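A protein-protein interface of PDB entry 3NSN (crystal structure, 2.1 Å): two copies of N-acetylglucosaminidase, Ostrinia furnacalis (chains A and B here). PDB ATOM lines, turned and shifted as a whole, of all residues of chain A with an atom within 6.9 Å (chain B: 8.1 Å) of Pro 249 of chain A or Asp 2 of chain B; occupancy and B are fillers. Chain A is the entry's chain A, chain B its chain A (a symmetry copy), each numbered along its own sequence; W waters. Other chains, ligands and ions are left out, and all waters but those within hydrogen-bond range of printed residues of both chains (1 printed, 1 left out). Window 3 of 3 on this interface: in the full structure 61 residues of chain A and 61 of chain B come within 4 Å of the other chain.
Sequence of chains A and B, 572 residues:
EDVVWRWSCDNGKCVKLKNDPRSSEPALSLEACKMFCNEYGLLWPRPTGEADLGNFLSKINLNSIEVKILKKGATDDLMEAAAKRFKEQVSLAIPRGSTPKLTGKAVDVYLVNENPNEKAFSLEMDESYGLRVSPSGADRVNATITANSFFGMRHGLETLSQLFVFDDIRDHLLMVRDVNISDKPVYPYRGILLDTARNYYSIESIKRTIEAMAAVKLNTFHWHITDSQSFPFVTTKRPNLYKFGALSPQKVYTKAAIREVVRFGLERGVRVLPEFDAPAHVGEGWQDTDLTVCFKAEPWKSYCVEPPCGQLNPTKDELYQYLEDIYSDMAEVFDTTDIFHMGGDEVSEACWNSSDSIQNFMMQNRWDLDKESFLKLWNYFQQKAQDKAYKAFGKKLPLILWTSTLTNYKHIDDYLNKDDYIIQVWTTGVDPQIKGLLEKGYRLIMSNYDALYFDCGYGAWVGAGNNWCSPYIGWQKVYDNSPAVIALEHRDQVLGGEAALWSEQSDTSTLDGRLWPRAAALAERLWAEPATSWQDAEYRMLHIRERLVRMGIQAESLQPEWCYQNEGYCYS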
ATOM      1  N   TYR A 242      13.604  24.808  -6.329  1.00  0.00           N
ATOM      2  CA  TYR A 242      14.501  23.654  -6.289  1.00  0.00           C
ATOM      3  C   TYR A 242      15.883  23.901  -6.875  1.00  0.00           C
ATOM      4  O   TYR A 242      16.847  23.441  -6.354  1.00  0.00           O
ATOM      5  CB  TYR A 242      13.873  22.390  -6.796  1.00  0.00           C
ATOM      6  CG  TYR A 242      13.766  22.192  -8.273  1.00  0.00           C
ATOM      7  CD1 TYR A 242      14.754  21.567  -8.965  1.00  0.00           C
ATOM      8  CD2 TYR A 242      12.639  22.558  -8.960  1.00  0.00           C
ATOM      9  CE1 TYR A 242      14.649  21.364 -10.268  1.00  0.00           C
ATOM     10  CE2 TYR A 242      12.526  22.346 -10.250  1.00  0.00           C
ATOM     11  CZ  TYR A 242      13.535  21.750 -10.918  1.00  0.00           C
ATOM     12  OH  TYR A 242      13.477  21.521 -12.234  1.00  0.00           O
ATOM     13  N   LYS A 243      15.930  24.654  -7.973  1.00  0.00           N
ATOM     14  CA  LYS A 243      17.181  24.914  -8.606  1.00  0.00           C
ATOM     15  C   LYS A 243      18.108  25.675  -7.745  1.00  0.00           C
ATOM     16  O   LYS A 243      19.199  25.304  -7.623  1.00  0.00           O
ATOM     17  CB  LYS A 243      17.002  25.640  -9.918  1.00  0.00           C
ATOM     18  CG  LYS A 243      16.570  24.761 -11.014  1.00  0.00           C
ATOM     19  CD  LYS A 243      16.125  25.543 -12.189  1.00  0.00           C
ATOM     20  CE  LYS A 243      16.353  24.830 -13.472  1.00  0.00           C
ATOM     21  NZ  LYS A 243      15.336  23.830 -13.818  1.00  0.00           N
ATOM     22  N   ALA A 246      18.211  23.277  -3.795  1.00  0.00           N
ATOM     23  CA  ALA A 246      18.796  21.980  -3.571  1.00  0.00           C
ATOM     24  C   ALA A 246      20.237  22.019  -3.143  1.00  0.00           C
ATOM     25  O   ALA A 246      20.944  22.905  -3.456  1.00  0.00           O
ATOM     26  CB  ALA A 246      18.635  21.153  -4.706  1.00  0.00           C
ATOM     27  N   LEU A 247      20.628  21.023  -2.385  1.00  0.00           N
ATOM     28  CA  LEU A 247      21.983  20.839  -1.948  1.00  0.00           C
ATOM     29  C   LEU A 247      22.872  20.619  -3.156  1.00  0.00           C
ATOM     30  O   LEU A 247      23.970  21.036  -3.173  1.00  0.00           O
ATOM     31  CB  LEU A 247      22.095  19.766  -0.879  1.00  0.00           C
ATOM     32  CG  LEU A 247      21.534  20.200   0.472  1.00  0.00           C
ATOM     33  CD1 LEU A 247      21.417  19.026   1.393  1.00  0.00           C
ATOM     34  CD2 LEU A 247      22.389  21.307   1.031  1.00  0.00           C
ATOM     35  N   SER A 248      22.334  19.974  -4.166  1.00  0.00           N
ATOM     36  CA  SER A 248      22.976  19.753  -5.424  1.00  0.00           C
ATOM     37  C   SER A 248      21.925  19.343  -6.404  1.00  0.00           C
ATOM     38  O   SER A 248      20.857  19.045  -6.030  1.00  0.00           O
ATOM     39  CB  SER A 248      24.089  18.713  -5.337  1.00  0.00           C
ATOM     40  OG  SER A 248      23.612  17.430  -5.550  1.00  0.00           O
ATOM     41  N   PRO A 249      22.260  19.317  -7.674  1.00  0.00           N
ATOM     42  CA  PRO A 249      21.313  18.967  -8.714  1.00  0.00           C
ATOM     43  C   PRO A 249      20.803  17.560  -8.573  1.00  0.00           C
ATOM     44  O   PRO A 249      19.732  17.335  -8.956  1.00  0.00           O
ATOM     45  CB  PRO A 249      22.135  19.132  -9.979  1.00  0.00           C
ATOM     46  CG  PRO A 249      23.107  20.054  -9.649  1.00  0.00           C
ATOM     47  CD  PRO A 249      23.504  19.782  -8.263  1.00  0.00           C
ATOM     48  N   GLN A 250      21.647  16.664  -8.117  1.00  0.00           N
ATOM     49  CA  GLN A 250      21.338  15.295  -7.758  1.00  0.00           C
ATOM     50  C   GLN A 250      20.444  15.121  -6.534  1.00  0.00           C
ATOM     51  O   GLN A 250      19.711  14.189  -6.467  1.00  0.00           O
ATOM     52  CB  GLN A 250      22.601  14.477  -7.535  1.00  0.00           C
ATOM     53  CG  GLN A 250      23.353  14.167  -8.740  1.00  0.00           C
ATOM     54  CD  GLN A 250      23.921  15.385  -9.380  1.00  0.00           C
ATOM     55  OE1 GLN A 250      24.603  16.199  -8.748  1.00  0.00           O
ATOM     56  NE2 GLN A 250      23.620  15.545 -10.643  1.00  0.00           N
ATOM     57  N   LYS A 251      20.588  15.987  -5.558  1.00  0.00           N
ATOM     58  CA  LYS A 251      19.853  15.857  -4.320  1.00  0.00           C
ATOM     59  C   LYS A 251      18.487  16.540  -4.382  1.00  0.00           C
ATOM     60  O   LYS A 251      18.262  17.535  -3.805  1.00  0.00           O
ATOM     61  CB  LYS A 251      20.704  16.332  -3.177  1.00  0.00           C
ATOM     62  CG  LYS A 251      21.845  15.455  -2.920  1.00  0.00           C
ATOM     63  CD  LYS A 251      22.755  15.993  -1.900  1.00  0.00           C
ATOM     64  CE  LYS A 251      23.841  15.007  -1.622  1.00  0.00           C
ATOM     65  NZ  LYS A 251      24.691  15.418  -0.535  1.00  0.00           N
ATOM     66  N   VAL A 252      17.596  15.924  -5.111  1.00  0.00           N
ATOM     67  CA  VAL A 252      16.339  16.465  -5.447  1.00  0.00           C
ATOM     68  C   VAL A 252      15.335  15.322  -5.463  1.00  0.00           C
ATOM     69  O   VAL A 252      15.709  14.223  -5.570  1.00  0.00           O
ATOM     70  CB  VAL A 252      16.581  17.093  -6.822  1.00  0.00           C
ATOM     71  CG1 VAL A 252      15.912  16.445  -7.918  1.00  0.00           C
ATOM     72  CG2 VAL A 252      16.606  18.543  -6.789  1.00  0.00           C
ATOM     73  N   GLU B   1      20.258  18.442 -13.539  1.00  0.00           N
ATOM     74  CA  GLU B   1      20.854  19.631 -14.109  1.00  0.00           C
ATOM     75  C   GLU B   1      22.278  20.021 -13.620  1.00  0.00           C
ATOM     76  O   GLU B   1      23.107  19.158 -13.389  1.00  0.00           O
ATOM     77  CB  GLU B   1      19.857  20.784 -14.097  1.00  0.00           C
ATOM     78  CG  GLU B   1      18.665  20.664 -13.148  1.00  0.00           C
ATOM     79  CD  GLU B   1      18.920  21.364 -11.862  1.00  0.00           C
ATOM     80  OE1 GLU B   1      18.421  20.940 -10.787  1.00  0.00           O
ATOM     81  OE2 GLU B   1      19.650  22.350 -11.934  1.00  0.00           O
ATOM     82  N   ASP B   2      22.559  21.309 -13.494  1.00  0.00           N
ATOM     83  CA  ASP B   2      23.904  21.815 -13.253  1.00  0.00           C
ATOM     84  C   ASP B   2      23.999  22.635 -12.009  1.00  0.00           C
ATOM     85  O   ASP B   2      23.070  23.326 -11.694  1.00  0.00           O
ATOM     86  CB  ASP B   2      24.274  22.796 -14.377  1.00  0.00           C
ATOM     87  CG  ASP B   2      24.367  22.154 -15.732  1.00  0.00           C
ATOM     88  OD1 ASP B   2      23.862  22.768 -16.684  1.00  0.00           O
ATOM     89  OD2 ASP B   2      24.970  21.063 -15.857  1.00  0.00           O
ATOM     90  N   VAL B   3      25.136  22.625 -11.334  1.00  0.00           N
ATOM     91  CA  VAL B   3      25.262  23.479 -10.200  1.00  0.00           C
ATOM     92  C   VAL B   3      25.163  24.928 -10.572  1.00  0.00           C
ATOM     93  O   VAL B   3      25.687  25.389 -11.548  1.00  0.00           O
ATOM     94  CB  VAL B   3      26.423  23.114  -9.260  1.00  0.00           C
ATOM     95  CG1 VAL B   3      27.205  22.074  -9.832  1.00  0.00           C
ATOM     96  CG2 VAL B   3      27.218  24.268  -8.849  1.00  0.00           C
ATOM     97  N   VAL B   4      24.394  25.592  -9.760  1.00  0.00           N
ATOM     98  CA  VAL B   4      24.008  26.957  -9.868  1.00  0.00           C
ATOM     99  C   VAL B   4      24.808  27.947  -9.064  1.00  0.00           C
ATOM    100  O   VAL B   4      24.662  29.107  -9.259  1.00  0.00           O
ATOM    101  CB  VAL B   4      22.545  26.973  -9.369  1.00  0.00           C
ATOM    102  CG1 VAL B   4      22.210  28.192  -8.738  1.00  0.00           C
ATOM    103  CG2 VAL B   4      21.629  26.691 -10.481  1.00  0.00           C
ATOM    104  N   TRP B   5      25.631  27.474  -8.149  1.00  0.00           N
ATOM    105  CA  TRP B   5      26.325  28.294  -7.199  1.00  0.00           C
ATOM    106  C   TRP B   5      27.845  28.234  -7.383  1.00  0.00           C
ATOM    107  O   TRP B   5      28.354  27.377  -8.010  1.00  0.00           O
ATOM    108  CB  TRP B   5      25.966  27.923  -5.741  1.00  0.00           C
ATOM    109  CG  TRP B   5      24.512  27.992  -5.364  1.00  0.00           C
ATOM    110  CD1 TRP B   5      23.646  26.978  -5.307  1.00  0.00           C
ATOM    111  CD2 TRP B   5      23.784  29.144  -4.993  1.00  0.00           C
ATOM    112  NE1 TRP B   5      22.432  27.404  -4.950  1.00  0.00           N
ATOM    113  CE2 TRP B   5      22.481  28.741  -4.740  1.00  0.00           C
ATOM    114  CE3 TRP B   5      24.103  30.484  -4.856  1.00  0.00           C
ATOM    115  CZ2 TRP B   5      21.503  29.619  -4.351  1.00  0.00           C
ATOM    116  CZ3 TRP B   5      23.128  31.355  -4.476  1.00  0.00           C
ATOM    117  CH2 TRP B   5      21.845  30.919  -4.228  1.00  0.00           C
ATOM    118  N   ASP B 168      32.753  20.005  -9.766  1.00  0.00           N
ATOM    119  CA  ASP B 168      31.449  19.622 -10.227  1.00  0.00           C
ATOM    120  C   ASP B 168      30.722  20.713 -11.028  1.00  0.00           C
ATOM    121  O   ASP B 168      29.697  20.474 -11.575  1.00  0.00           O
ATOM    122  CB  ASP B 168      30.621  19.091  -9.076  1.00  0.00           C
ATOM    123  CG  ASP B 168      30.421  20.098  -7.983  1.00  0.00           C
ATOM    124  OD1 ASP B 168      29.447  19.966  -7.315  1.00  0.00           O
ATOM    125  OD2 ASP B 168      31.220  20.977  -7.735  1.00  0.00           O
ATOM    126  N   ILE B 169      31.251  21.919 -11.032  1.00  0.00           N
ATOM    127  CA  ILE B 169      30.805  22.915 -11.974  1.00  0.00           C
ATOM    128  C   ILE B 169      31.235  22.561 -13.407  1.00  0.00           C
ATOM    129  O   ILE B 169      30.458  22.572 -14.276  1.00  0.00           O
ATOM    130  CB  ILE B 169      31.272  24.336 -11.631  1.00  0.00           C
ATOM    131  CG1 ILE B 169      30.671  24.795 -10.322  1.00  0.00           C
ATOM    132  CG2 ILE B 169      30.874  25.252 -12.703  1.00  0.00           C
ATOM    133  CD1 ILE B 169      31.138  26.050  -9.855  1.00  0.00           C
ATOM    134  N   ARG B 170      32.497  22.238 -13.617  1.00  0.00           N
ATOM    135  CA  ARG B 170      32.991  21.896 -14.922  1.00  0.00           C
ATOM    136  C   ARG B 170      33.092  20.416 -15.296  1.00  0.00           C
ATOM    137  O   ARG B 170      33.259  20.090 -16.411  1.00  0.00           O
ATOM    138  CB  ARG B 170      34.333  22.550 -15.093  1.00  0.00           C
ATOM    139  CG  ARG B 170      34.246  24.022 -15.092  1.00  0.00           C
ATOM    140  CD  ARG B 170      35.567  24.675 -14.978  1.00  0.00           C
ATOM    141  NE  ARG B 170      35.439  26.102 -14.808  1.00  0.00           N
ATOM    142  CZ  ARG B 170      35.430  26.749 -13.672  1.00  0.00           C
ATOM    143  NH1 ARG B 170      35.366  28.045 -13.685  1.00  0.00           N
ATOM    144  NH2 ARG B 170      35.184  26.123 -12.538  1.00  0.00           N
ATOM    145  N   ASP B 171      32.933  19.545 -14.322  1.00  0.00           N
ATOM    146  CA  ASP B 171      33.251  18.128 -14.388  1.00  0.00           C
ATOM    147  C   ASP B 171      34.733  17.811 -14.666  1.00  0.00           C
ATOM    148  O   ASP B 171      35.041  17.024 -15.468  1.00  0.00           O
ATOM    149  CB  ASP B 171      32.356  17.391 -15.342  1.00  0.00           C
ATOM    150  CG  ASP B 171      30.937  17.309 -14.882  1.00  0.00           C
ATOM    151  OD1 ASP B 171      30.678  17.144 -13.701  1.00  0.00           O
ATOM    152  OD2 ASP B 171      30.057  17.354 -15.716  1.00  0.00           O
ATOM    153  N   GLN B 565      28.377  23.738   3.184  1.00  0.00           N
ATOM    154  CA  GLN B 565      28.276  24.650   2.079  1.00  0.00           C
ATOM    155  C   GLN B 565      28.328  26.119   2.477  1.00  0.00           C
ATOM    156  O   GLN B 565      28.567  26.926   1.671  1.00  0.00           O
ATOM    157  CB  GLN B 565      27.022  24.359   1.264  1.00  0.00           C
ATOM    158  CG  GLN B 565      27.035  23.032   0.610  1.00  0.00           C
ATOM    159  CD  GLN B 565      25.972  22.856  -0.413  1.00  0.00           C
ATOM    160  OE1 GLN B 565      25.147  23.669  -0.602  1.00  0.00           O
ATOM    161  NE2 GLN B 565      25.982  21.761  -1.032  1.00  0.00           N
HETATM  162  O   HOH W   1      21.342  24.620  -5.613  1.00  0.00           O
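The backbone carbonyl oxygen (O) of Leu 247 of chain A lies within hydrogen-bond range of the side-chain amide nitrogen (NE2) of Gln 565 of chain B (3.0 Å).
OH of Tyr 242 of chain A lies within hydrogen-bond range of NZ of Lys 243 of chain A (3.4 Å).
OE1 of Glu 1 of chain B touches CE1 of Tyr 242 of chain A (3.8 Å).
Lys 243 of chain A touches Val 4 of chain B.
CB of Pro 249 of chain A touches O of Glu 1 of chain B (3.5 Å).
CG of Pro 249 of chain A touches C of Asp 2 of chain B, 3.6 Å away.
Pro 249 of chain A touches Val 3 of chain B.
No residue of chain B comes within 4 Å of Ser 248 of chain A.
Of chain B, only Glu 1 (3.5 Å), Asp 2 (3.6 Å) and Val 3 (3.7 Å) come within 4 Å of Pro 249 of chain A.
Gln 250 of chain A touches none of the printed residues of chain B.
Of the printed residues of chain A, Glu 1 of chain B touches Tyr 242 (3.8 Å) and Pro 249 (3.5 Å).
Asp 2 of chain B touches just one residue of chain A: Pro 249 (3.6 Å).
Trp 5 of chain B touches none of the printed residues of chain A.
Of the printed residues of chain A, Gln 565 of chain B touches Leu 247.
The nearest residue of chain A that does not touch Asp 2 of chain B is Lys 243 of chain A (6.0 Å).
The nearest printed residue of chain B that does not touch Tyr 242 of chain A is Trp 5 of chain B (7.0 Å).
Of the 9 printed residues of chain A, 4 touch a printed residue of chain B.
Printed residues of chain B that touch a printed residue of chain A: Glu 1, Asp 2, Val 3, Val 4 and Gln 565.
Hydrophobic or aromatic side chains of chain B that line the printed part of chain A: Val 4.
No position is printed for both chains.
Water W1 lies within hydrogen-bond range of O of Ala 246 of chain A, O of Lys 243 of chain A and NE1 of Trp 5 of chain B.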
